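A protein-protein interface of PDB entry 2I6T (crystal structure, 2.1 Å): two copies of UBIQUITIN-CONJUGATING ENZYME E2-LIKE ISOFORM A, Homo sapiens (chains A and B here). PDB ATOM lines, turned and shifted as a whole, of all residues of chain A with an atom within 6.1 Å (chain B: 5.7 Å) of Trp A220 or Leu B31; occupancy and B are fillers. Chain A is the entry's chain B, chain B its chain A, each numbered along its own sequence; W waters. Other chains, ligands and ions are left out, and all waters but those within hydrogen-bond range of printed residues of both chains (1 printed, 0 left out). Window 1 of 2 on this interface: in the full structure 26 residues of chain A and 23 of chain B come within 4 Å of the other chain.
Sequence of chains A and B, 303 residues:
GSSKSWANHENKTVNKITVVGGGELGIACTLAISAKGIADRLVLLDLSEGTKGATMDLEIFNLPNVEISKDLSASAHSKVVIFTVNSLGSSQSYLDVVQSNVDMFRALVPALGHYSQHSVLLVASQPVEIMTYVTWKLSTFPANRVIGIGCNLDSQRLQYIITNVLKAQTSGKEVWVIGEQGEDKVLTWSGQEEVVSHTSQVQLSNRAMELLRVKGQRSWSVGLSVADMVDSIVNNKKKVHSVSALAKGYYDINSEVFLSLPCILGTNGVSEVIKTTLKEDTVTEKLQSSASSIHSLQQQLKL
Glu B24 touches its own counterpart, Glu A24. Ala A35 touches Leu B31, but with the chains exchanged Leu A31 does not touch Ala B35 (4.7 Å). Ala B35 touches its own counterpart, Ala A35. Trp B220 touches its own counterpart, Trp A220. Of the 15 pairs that touch across the chains among the printed residues, 7 have their exchanged pair printed and touching as well.
Among the printed residues, merely in contact across the chains: Ile A27 with Trp B220 (3.5 Å), Ala A32 with Phe B61 (3.3 Å), Ser A34 with Ala B35 (3.9 Å), Ala A35 with Leu B31 (3.6 Å), Ala A35 with Ser B34 (3.98 Å), Ala A35 with Ala B35 (3.7 Å), Ala A35 with Leu B63 (3.7 Å), Leu A63 with Ala B35 (3.6 Å), Trp A220 with Leu B31 (3.6 Å), Trp A220 with Trp B220 (3.7 Å), Ser A221 with Ala B54 (3.4 Å), Leu A224 with Leu B58 (3.9 Å) and Leu A224 with Phe B61 (3.5 Å).
Leu B31 touches just these residues of chain A: Ala A35 and Trp A220. Of the printed residues of chain B, Ser A34 touches Ala B35. Printed residues of chain A within 4 Å of Leu B58: Leu A224. Printed residues of chain B within 4 Å of Leu A224: Leu B58 and Phe B61. Of the printed residues of chain B, Ser A221 touches Ala B54. Of the printed residues of chain A, Trp B220 touches Ile A27 (3.5 Å) and Trp A220 (3.7 Å). Cys B29 touches none of the printed residues of chain A. The nearest residue of chain A that does not touch Leu B31 is Leu A31 (4.1 Å).
OE2 of Glu A24 lies close to OG of Ser A219 (3.3 Å). O of Thr B30 is in hydrogen-bond range of OG of Ser B34 (2.6 Å). The side-chain hydroxyl (OG) of Ser B219 sits close to the side-chain carboxylate (OE1) of Glu B24 (3.2 Å).
Water W1 lies within hydrogen-bond range of the guanidinium group (NH1) of Arg A218 and the backbone NH (N) of Glu B24.
OE2 of Glu B24 sits close to NE1 of Trp A220 (3.0 Å). OE2 of Glu A24 lies close to OE2 of Glu B24 (3.1 Å).
Hydrophobic or aromatic side chains of chain A within 4 Å of the printed part of chain B: Ile A27, Ala A35, Leu A63, Trp A220 and Leu A224. Hydrophobic or aromatic side chains of chain B that line the printed part of chain A: Leu B31, Ala B35, Ala B54, Leu B58, Phe B61, Leu B63 and Trp B220. Among the printed residues, 15 pairs touch across the chains.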
ATOM      1  N   GLU A  24       2.569 -11.332  12.569  1.00  0.00           N
ATOM      2  CA  GLU A  24       1.639 -12.330  13.115  1.00  0.00           C
ATOM      3  C   GLU A  24       2.250 -13.742  13.153  1.00  0.00           C
ATOM      4  O   GLU A  24       2.172 -14.445  14.184  1.00  0.00           O
ATOM      5  CB  GLU A  24       0.337 -12.332  12.305  1.00  0.00           C
ATOM      6  CG  GLU A  24      -0.835 -12.986  13.022  1.00  0.00           C
ATOM      7  CD  GLU A  24      -2.110 -12.989  12.184  1.00  0.00           C
ATOM      8  OE1 GLU A  24      -2.562 -11.890  11.764  1.00  0.00           O
ATOM      9  OE2 GLU A  24      -2.670 -14.088  11.954  1.00  0.00           O
ATOM     10  N   LEU A  25       2.873 -14.137  12.037  1.00  0.00           N
ATOM     11  CA  LEU A  25       3.456 -15.477  11.943  1.00  0.00           C
ATOM     12  C   LEU A  25       4.446 -15.700  13.071  1.00  0.00           C
ATOM     13  O   LEU A  25       4.364 -16.687  13.779  1.00  0.00           O
ATOM     14  CB  LEU A  25       4.114 -15.713  10.590  1.00  0.00           C
ATOM     15  CG  LEU A  25       4.572 -17.151  10.316  1.00  0.00           C
ATOM     16  CD1 LEU A  25       3.567 -18.207  10.810  1.00  0.00           C
ATOM     17  CD2 LEU A  25       4.857 -17.289   8.827  1.00  0.00           C
ATOM     18  N   ILE A  27       4.853 -14.096  15.996  1.00  0.00           N
ATOM     19  CA  ILE A  27       4.196 -14.210  17.312  1.00  0.00           C
ATOM     20  C   ILE A  27       3.503 -15.569  17.457  1.00  0.00           C
ATOM     21  O   ILE A  27       3.656 -16.239  18.491  1.00  0.00           O
ATOM     22  CB  ILE A  27       3.220 -13.005  17.632  1.00  0.00           C
ATOM     23  CG1 ILE A  27       4.023 -11.744  17.932  1.00  0.00           C
ATOM     24  CG2 ILE A  27       2.322 -13.291  18.844  1.00  0.00           C
ATOM     25  CD1 ILE A  27       4.031 -10.785  16.784  1.00  0.00           C
ATOM     26  N   ALA A  28       2.766 -15.981  16.424  1.00  0.00           N
ATOM     27  CA  ALA A  28       2.107 -17.306  16.443  1.00  0.00           C
ATOM     28  C   ALA A  28       3.107 -18.420  16.739  1.00  0.00           C
ATOM     29  O   ALA A  28       2.839 -19.254  17.604  1.00  0.00           O
ATOM     30  CB  ALA A  28       1.372 -17.584  15.159  1.00  0.00           C
ATOM     31  N   CYS A  29       4.266 -18.420  16.054  1.00  0.00           N
ATOM     32  CA  CYS A  29       5.318 -19.409  16.359  1.00  0.00           C
ATOM     33  C   CYS A  29       5.773 -19.321  17.795  1.00  0.00           C
ATOM     34  O   CYS A  29       5.947 -20.331  18.487  1.00  0.00           O
ATOM     35  CB  CYS A  29       6.531 -19.268  15.418  1.00  0.00           C
ATOM     36  SG  CYS A  29       6.129 -19.648  13.708  1.00  0.00           S
ATOM     37  N   LEU A  31       4.220 -17.959  20.499  1.00  0.00           N
ATOM     38  CA  LEU A  31       3.196 -18.389  21.482  1.00  0.00           C
ATOM     39  C   LEU A  31       3.052 -19.902  21.497  1.00  0.00           C
ATOM     40  O   LEU A  31       3.022 -20.513  22.582  1.00  0.00           O
ATOM     41  CB  LEU A  31       1.843 -17.702  21.240  1.00  0.00           C
ATOM     42  CG  LEU A  31       1.788 -16.314  21.911  1.00  0.00           C
ATOM     43  CD1 LEU A  31       0.560 -15.511  21.461  1.00  0.00           C
ATOM     44  CD2 LEU A  31       1.788 -16.495  23.402  1.00  0.00           C
ATOM     45  N   ALA A  32       3.002 -20.507  20.300  1.00  0.00           N
ATOM     46  CA  ALA A  32       2.924 -21.985  20.185  1.00  0.00           C
ATOM     47  C   ALA A  32       4.089 -22.675  20.877  1.00  0.00           C
ATOM     48  O   ALA A  32       3.895 -23.615  21.618  1.00  0.00           O
ATOM     49  CB  ALA A  32       2.842 -22.428  18.711  1.00  0.00           C
ATOM     50  N   SER A  34       6.116 -21.514  23.345  1.00  0.00           N
ATOM     51  CA  SER A  34       5.986 -21.248  24.785  1.00  0.00           C
ATOM     52  C   SER A  34       4.882 -22.056  25.409  1.00  0.00           C
ATOM     53  O   SER A  34       5.100 -22.665  26.460  1.00  0.00           O
ATOM     54  CB  SER A  34       5.682 -19.776  25.065  1.00  0.00           C
ATOM     55  OG  SER A  34       6.718 -18.998  24.566  1.00  0.00           O
ATOM     56  N   ALA A  35       3.711 -22.070  24.758  1.00  0.00           N
ATOM     57  CA  ALA A  35       2.553 -22.845  25.270  1.00  0.00           C
ATOM     58  C   ALA A  35       2.921 -24.283  25.673  1.00  0.00           C
ATOM     59  O   ALA A  35       2.379 -24.814  26.633  1.00  0.00           O
ATOM     60  CB  ALA A  35       1.401 -22.830  24.262  1.00  0.00           C
ATOM     61  N   LEU A  63       5.817 -13.364  29.014  1.00  0.00           N
ATOM     62  CA  LEU A  63       5.846 -14.737  28.491  1.00  0.00           C
ATOM     63  C   LEU A  63       7.139 -15.363  28.939  1.00  0.00           C
ATOM     64  O   LEU A  63       8.194 -14.783  28.714  1.00  0.00           O
ATOM     65  CB  LEU A  63       5.811 -14.724  26.974  1.00  0.00           C
ATOM     66  CG  LEU A  63       4.491 -14.817  26.242  1.00  0.00           C
ATOM     67  CD1 LEU A  63       4.838 -15.090  24.803  1.00  0.00           C
ATOM     68  CD2 LEU A  63       3.657 -15.950  26.803  1.00  0.00           C
ATOM     69  N   ARG A 218      -3.635 -20.375   7.866  1.00  0.00           N
ATOM     70  CA  ARG A 218      -3.558 -19.170   8.699  1.00  0.00           C
ATOM     71  C   ARG A 218      -2.392 -19.216   9.683  1.00  0.00           C
ATOM     72  O   ARG A 218      -1.894 -20.298  10.030  1.00  0.00           O
ATOM     73  CB  ARG A 218      -4.900 -18.907   9.397  1.00  0.00           C
ATOM     74  CG  ARG A 218      -6.003 -18.503   8.381  1.00  0.00           C
ATOM     75  CD  ARG A 218      -7.344 -18.190   9.032  1.00  0.00           C
ATOM     76  NE  ARG A 218      -7.333 -16.869   9.659  1.00  0.00           N
ATOM     77  CZ  ARG A 218      -8.327 -16.372  10.391  1.00  0.00           C
ATOM     78  NH1 ARG A 218      -9.436 -17.077  10.602  1.00  0.00           N
ATOM     79  NH2 ARG A 218      -8.210 -15.159  10.919  1.00  0.00           N
ATOM     80  N   SER A 219      -1.957 -18.032  10.114  1.00  0.00           N
ATOM     81  CA  SER A 219      -0.727 -17.866  10.901  1.00  0.00           C
ATOM     82  C   SER A 219      -0.669 -18.756  12.124  1.00  0.00           C
ATOM     83  O   SER A 219       0.388 -19.294  12.466  1.00  0.00           O
ATOM     84  CB  SER A 219      -0.584 -16.405  11.348  1.00  0.00           C
ATOM     85  OG  SER A 219      -0.305 -15.585  10.231  1.00  0.00           O
ATOM     86  N   TRP A 220      -1.813 -18.886  12.798  1.00  0.00           N
ATOM     87  CA  TRP A 220      -1.869 -19.652  14.035  1.00  0.00           C
ATOM     88  C   TRP A 220      -1.674 -21.120  13.739  1.00  0.00           C
ATOM     89  O   TRP A 220      -1.007 -21.796  14.482  1.00  0.00           O
ATOM     90  CB  TRP A 220      -3.144 -19.333  14.844  1.00  0.00           C
ATOM     91  CG  TRP A 220      -3.065 -17.882  15.315  1.00  0.00           C
ATOM     92  CD1 TRP A 220      -3.543 -16.781  14.647  1.00  0.00           C
ATOM     93  CD2 TRP A 220      -2.362 -17.369  16.476  1.00  0.00           C
ATOM     94  NE1 TRP A 220      -3.216 -15.630  15.338  1.00  0.00           N
ATOM     95  CE2 TRP A 220      -2.502 -15.963  16.464  1.00  0.00           C
ATOM     96  CE3 TRP A 220      -1.653 -17.967  17.529  1.00  0.00           C
ATOM     97  CZ2 TRP A 220      -1.949 -15.143  17.456  1.00  0.00           C
ATOM     98  CZ3 TRP A 220      -1.119 -17.155  18.522  1.00  0.00           C
ATOM     99  CH2 TRP A 220      -1.273 -15.758  18.479  1.00  0.00           C
ATOM    100  N   SER A 221      -2.219 -21.594  12.626  1.00  0.00           N
ATOM    101  CA  SER A 221      -2.066 -22.997  12.244  1.00  0.00           C
ATOM    102  C   SER A 221      -0.592 -23.277  11.939  1.00  0.00           C
ATOM    103  O   SER A 221       0.002 -24.262  12.452  1.00  0.00           O
ATOM    104  CB  SER A 221      -2.907 -23.301  11.011  1.00  0.00           C
ATOM    105  OG  SER A 221      -4.297 -23.197  11.306  1.00  0.00           O
ATOM    106  N   VAL A 222      -0.006 -22.398  11.130  1.00  0.00           N
ATOM    107  CA  VAL A 222       1.385 -22.544  10.717  1.00  0.00           C
ATOM    108  C   VAL A 222       2.341 -22.513  11.911  1.00  0.00           C
ATOM    109  O   VAL A 222       3.305 -23.292  11.968  1.00  0.00           O
ATOM    110  CB  VAL A 222       1.789 -21.507   9.674  1.00  0.00           C
ATOM    111  CG1 VAL A 222       3.308 -21.592   9.411  1.00  0.00           C
ATOM    112  CG2 VAL A 222       1.002 -21.742   8.363  1.00  0.00           C
ATOM    113  N   GLY A 223       2.078 -21.603  12.849  1.00  0.00           N
ATOM    114  CA  GLY A 223       2.857 -21.523  14.071  1.00  0.00           C
ATOM    115  C   GLY A 223       2.820 -22.777  14.926  1.00  0.00           C
ATOM    116  O   GLY A 223       3.822 -23.117  15.540  1.00  0.00           O
ATOM    117  N   LEU A 224       1.662 -23.446  14.993  1.00  0.00           N
ATOM    118  CA  LEU A 224       1.551 -24.734  15.683  1.00  0.00           C
ATOM    119  C   LEU A 224       2.360 -25.776  14.951  1.00  0.00           C
ATOM    120  O   LEU A 224       3.074 -26.573  15.570  1.00  0.00           O
ATOM    121  CB  LEU A 224       0.077 -25.186  15.825  1.00  0.00           C
ATOM    122  CG  LEU A 224      -0.771 -24.237  16.705  1.00  0.00           C
ATOM    123  CD1 LEU A 224      -2.274 -24.444  16.520  1.00  0.00           C
ATOM    124  CD2 LEU A 224      -0.384 -24.358  18.171  1.00  0.00           C
ATOM    125  N   SER A 225       2.277 -25.759  13.631  1.00  0.00           N
ATOM    126  CA  SER A 225       3.044 -26.710  12.810  1.00  0.00           C
ATOM    127  C   SER A 225       4.559 -26.516  13.051  1.00  0.00           C
ATOM    128  O   SER A 225       5.317 -27.480  13.327  1.00  0.00           O
ATOM    129  CB  SER A 225       2.667 -26.538  11.340  1.00  0.00           C
ATOM    130  OG  SER A 225       3.639 -27.097  10.470  1.00  0.00           O
ATOM    131  N   GLU B  24      -9.182 -16.779  15.598  1.00  0.00           N
ATOM    132  CA  GLU B  24      -7.832 -16.309  15.893  1.00  0.00           C
ATOM    133  C   GLU B  24      -7.660 -15.830  17.351  1.00  0.00           C
ATOM    134  O   GLU B  24      -6.701 -16.220  18.020  1.00  0.00           O
ATOM    135  CB  GLU B  24      -7.426 -15.198  14.907  1.00  0.00           C
ATOM    136  CG  GLU B  24      -6.032 -14.629  15.162  1.00  0.00           C
ATOM    137  CD  GLU B  24      -5.673 -13.362  14.336  1.00  0.00           C
ATOM    138  OE1 GLU B  24      -6.585 -12.665  13.801  1.00  0.00           O
ATOM    139  OE2 GLU B  24      -4.444 -13.068  14.247  1.00  0.00           O
ATOM    140  N   GLY B  26      -9.544 -16.616  20.034  1.00  0.00           N
ATOM    141  CA  GLY B  26      -9.697 -17.767  20.933  1.00  0.00           C
ATOM    142  C   GLY B  26      -8.429 -18.590  21.034  1.00  0.00           C
ATOM    143  O   GLY B  26      -8.047 -19.024  22.129  1.00  0.00           O
ATOM    144  N   ILE B  27      -7.791 -18.837  19.890  1.00  0.00           N
ATOM    145  CA  ILE B  27      -6.490 -19.510  19.850  1.00  0.00           C
ATOM    146  C   ILE B  27      -5.440 -18.675  20.596  1.00  0.00           C
ATOM    147  O   ILE B  27      -4.678 -19.199  21.406  1.00  0.00           O
ATOM    148  CB  ILE B  27      -5.982 -19.784  18.360  1.00  0.00           C
ATOM    149  CG1 ILE B  27      -7.005 -20.579  17.547  1.00  0.00           C
ATOM    150  CG2 ILE B  27      -4.639 -20.513  18.375  1.00  0.00           C
ATOM    151  CD1 ILE B  27      -7.269 -21.940  18.091  1.00  0.00           C
ATOM    152  N   ALA B  28      -5.388 -17.381  20.295  1.00  0.00           N
ATOM    153  CA  ALA B  28      -4.453 -16.460  20.978  1.00  0.00           C
ATOM    154  C   ALA B  28      -4.597 -16.544  22.489  1.00  0.00           C
ATOM    155  O   ALA B  28      -3.588 -16.684  23.212  1.00  0.00           O
ATOM    156  CB  ALA B  28      -4.661 -15.041  20.500  1.00  0.00           C
ATOM    157  N   CYS B  29      -5.845 -16.488  22.971  1.00  0.00           N
ATOM    158  CA  CYS B  29      -6.103 -16.607  24.407  1.00  0.00           C
ATOM    159  C   CYS B  29      -5.654 -17.950  24.982  1.00  0.00           C
ATOM    160  O   CYS B  29      -5.035 -18.007  26.061  1.00  0.00           O
ATOM    161  CB  CYS B  29      -7.603 -16.386  24.718  1.00  0.00           C
ATOM    162  SG  CYS B  29      -8.186 -14.713  24.388  1.00  0.00           S
ATOM    163  N   THR B  30      -5.986 -19.037  24.291  1.00  0.00           N
ATOM    164  CA  THR B  30      -5.630 -20.367  24.769  1.00  0.00           C
ATOM    165  C   THR B  30      -4.115 -20.556  24.923  1.00  0.00           C
ATOM    166  O   THR B  30      -3.619 -21.102  25.932  1.00  0.00           O
ATOM    167  CB  THR B  30      -6.201 -21.432  23.804  1.00  0.00           C
ATOM    168  OG1 THR B  30      -7.635 -21.286  23.727  1.00  0.00           O
ATOM    169  CG2 THR B  30      -5.859 -22.802  24.297  1.00  0.00           C
ATOM    170  N   LEU B  31      -3.379 -20.091  23.926  1.00  0.00           N
ATOM    171  CA  LEU B  31      -1.928 -20.219  23.903  1.00  0.00           C
ATOM    172  C   LEU B  31      -1.298 -19.338  24.948  1.00  0.00           C
ATOM    173  O   LEU B  31      -0.376 -19.795  25.648  1.00  0.00           O
ATOM    174  CB  LEU B  31      -1.364 -19.915  22.512  1.00  0.00           C
ATOM    175  CG  LEU B  31      -1.700 -20.928  21.394  1.00  0.00           C
ATOM    176  CD1 LEU B  31      -1.174 -20.490  20.024  1.00  0.00           C
ATOM    177  CD2 LEU B  31      -1.145 -22.276  21.732  1.00  0.00           C
ATOM    178  N   ALA B  32      -1.808 -18.104  25.097  1.00  0.00           N
ATOM    179  CA  ALA B  32      -1.267 -17.212  26.124  1.00  0.00           C
ATOM    180  C   ALA B  32      -1.499 -17.815  27.512  1.00  0.00           C
ATOM    181  O   ALA B  32      -0.575 -17.880  28.325  1.00  0.00           O
ATOM    182  CB  ALA B  32      -1.864 -15.841  26.023  1.00  0.00           C
ATOM    183  N   ILE B  33      -2.716 -18.310  27.757  1.00  0.00           N
ATOM    184  CA  ILE B  33      -3.048 -18.919  29.044  1.00  0.00           C
ATOM    185  C   ILE B  33      -2.155 -20.149  29.312  1.00  0.00           C
ATOM    186  O   ILE B  33      -1.585 -20.263  30.392  1.00  0.00           O
ATOM    187  CB  ILE B  33      -4.559 -19.264  29.140  1.00  0.00           C
ATOM    188  CG1 ILE B  33      -5.395 -17.981  29.194  1.00  0.00           C
ATOM    189  CG2 ILE B  33      -4.839 -20.092  30.395  1.00  0.00           C
ATOM    190  CD1 ILE B  33      -6.922 -18.183  28.989  1.00  0.00           C
ATOM    191  N   SER B  34      -2.033 -21.046  28.318  1.00  0.00           N
ATOM    192  CA  SER B  34      -1.194 -22.247  28.430  1.00  0.00           C
ATOM    193  C   SER B  34       0.259 -21.885  28.681  1.00  0.00           C
ATOM    194  O   SER B  34       0.901 -22.467  29.579  1.00  0.00           O
ATOM    195  CB  SER B  34      -1.290 -23.116  27.182  1.00  0.00           C
ATOM    196  OG  SER B  34      -2.650 -23.328  26.880  1.00  0.00           O
ATOM    197  N   ALA B  35       0.751 -20.895  27.934  1.00  0.00           N
ATOM    198  CA  ALA B  35       2.149 -20.433  28.038  1.00  0.00           C
ATOM    199  C   ALA B  35       2.524 -20.028  29.448  1.00  0.00           C
ATOM    200  O   ALA B  35       3.640 -20.300  29.879  1.00  0.00           O
ATOM    201  CB  ALA B  35       2.412 -19.292  27.090  1.00  0.00           C
ATOM    202  N   LYS B  36       1.574 -19.424  30.164  1.00  0.00           N
ATOM    203  CA  LYS B  36       1.806 -18.913  31.500  1.00  0.00           C
ATOM    204  C   LYS B  36       1.499 -19.948  32.587  1.00  0.00           C
ATOM    205  O   LYS B  36       1.779 -19.702  33.749  1.00  0.00           O
ATOM    206  CB  LYS B  36       0.985 -17.632  31.750  1.00  0.00           C
ATOM    207  CG  LYS B  36       1.247 -16.478  30.764  1.00  0.00           C
ATOM    208  CD  LYS B  36       2.434 -15.622  31.183  1.00  0.00           C
ATOM    209  CE  LYS B  36       2.037 -14.549  32.210  1.00  0.00           C
ATOM    210  NZ  LYS B  36       3.026 -14.462  33.327  1.00  0.00           N
ATOM    211  N   ALA B  54      -8.424 -24.104  12.122  1.00  0.00           N
ATOM    212  CA  ALA B  54      -7.308 -23.901  13.060  1.00  0.00           C
ATOM    213  C   ALA B  54      -7.538 -24.545  14.434  1.00  0.00           C
ATOM    214  O   ALA B  54      -6.604 -24.664  15.238  1.00  0.00           O
ATOM    215  CB  ALA B  54      -6.975 -22.408  13.219  1.00  0.00           C
ATOM    216  N   LEU B  58      -5.010 -27.257  16.865  1.00  0.00           N
ATOM    217  CA  LEU B  58      -4.705 -27.163  18.288  1.00  0.00           C
ATOM    218  C   LEU B  58      -4.889 -28.536  18.918  1.00  0.00           C
ATOM    219  O   LEU B  58      -4.115 -28.933  19.791  1.00  0.00           O
ATOM    220  CB  LEU B  58      -5.588 -26.115  18.965  1.00  0.00           C
ATOM    221  CG  LEU B  58      -5.074 -25.574  20.293  1.00  0.00           C
ATOM    222  CD1 LEU B  58      -3.777 -24.828  20.076  1.00  0.00           C
ATOM    223  CD2 LEU B  58      -6.103 -24.660  20.919  1.00  0.00           C
ATOM    224  N   PHE B  61      -1.779 -30.437  18.008  1.00  0.00           N
ATOM    225  CA  PHE B  61      -0.685 -29.955  18.836  1.00  0.00           C
ATOM    226  C   PHE B  61      -0.653 -30.568  20.248  1.00  0.00           C
ATOM    227  O   PHE B  61       0.417 -30.678  20.860  1.00  0.00           O
ATOM    228  CB  PHE B  61      -0.776 -28.432  18.933  1.00  0.00           C
ATOM    229  CG  PHE B  61       0.471 -27.771  19.451  1.00  0.00           C
ATOM    230  CD1 PHE B  61       1.706 -28.000  18.841  1.00  0.00           C
ATOM    231  CD2 PHE B  61       0.408 -26.878  20.529  1.00  0.00           C
ATOM    232  CE1 PHE B  61       2.864 -27.381  19.307  1.00  0.00           C
ATOM    233  CE2 PHE B  61       1.566 -26.231  21.001  1.00  0.00           C
ATOM    234  CZ  PHE B  61       2.794 -26.487  20.388  1.00  0.00           C
ATOM    235  N   LEU B  63      -1.806 -29.975  23.629  1.00  0.00           N
ATOM    236  CA  LEU B  63      -1.445 -29.344  24.902  1.00  0.00           C
ATOM    237  C   LEU B  63      -2.055 -30.106  26.090  1.00  0.00           C
ATOM    238  O   LEU B  63      -3.259 -30.408  26.086  1.00  0.00           O
ATOM    239  CB  LEU B  63      -1.921 -27.891  24.918  1.00  0.00           C
ATOM    240  CG  LEU B  63      -1.241 -26.925  23.952  1.00  0.00           C
ATOM    241  CD1 LEU B  63      -1.973 -25.591  23.877  1.00  0.00           C
ATOM    242  CD2 LEU B  63       0.218 -26.712  24.376  1.00  0.00           C
ATOM    243  N   SER B 219      -4.984  -9.624  17.809  1.00  0.00           N
ATOM    244  CA  SER B 219      -5.437 -10.819  18.513  1.00  0.00           C
ATOM    245  C   SER B 219      -4.505 -11.287  19.592  1.00  0.00           C
ATOM    246  O   SER B 219      -4.947 -11.620  20.689  1.00  0.00           O
ATOM    247  CB  SER B 219      -5.586 -11.981  17.537  1.00  0.00           C
ATOM    248  OG  SER B 219      -6.813 -11.885  16.853  1.00  0.00           O
ATOM    249  N   TRP B 220      -3.217 -11.362  19.269  1.00  0.00           N
ATOM    250  CA  TRP B 220      -2.265 -11.908  20.231  1.00  0.00           C
ATOM    251  C   TRP B 220      -2.064 -10.979  21.415  1.00  0.00           C
ATOM    252  O   TRP B 220      -1.873 -11.449  22.564  1.00  0.00           O
ATOM    253  CB  TRP B 220      -0.949 -12.269  19.555  1.00  0.00           C
ATOM    254  CG  TRP B 220      -0.593 -11.294  18.489  1.00  0.00           C
ATOM    255  CD1 TRP B 220      -1.011 -11.297  17.172  1.00  0.00           C
ATOM    256  CD2 TRP B 220       0.236 -10.145  18.650  1.00  0.00           C
ATOM    257  NE1 TRP B 220      -0.469 -10.211  16.504  1.00  0.00           N
ATOM    258  CE2 TRP B 220       0.296  -9.491  17.389  1.00  0.00           C
ATOM    259  CE3 TRP B 220       0.951  -9.612  19.733  1.00  0.00           C
ATOM    260  CZ2 TRP B 220       1.039  -8.330  17.190  1.00  0.00           C
ATOM    261  CZ3 TRP B 220       1.687  -8.464  19.540  1.00  0.00           C
ATOM    262  CH2 TRP B 220       1.731  -7.832  18.279  1.00  0.00           C
HETATM  263  O   HOH W   1     -10.982 -15.730  13.011  1.00  0.00           O
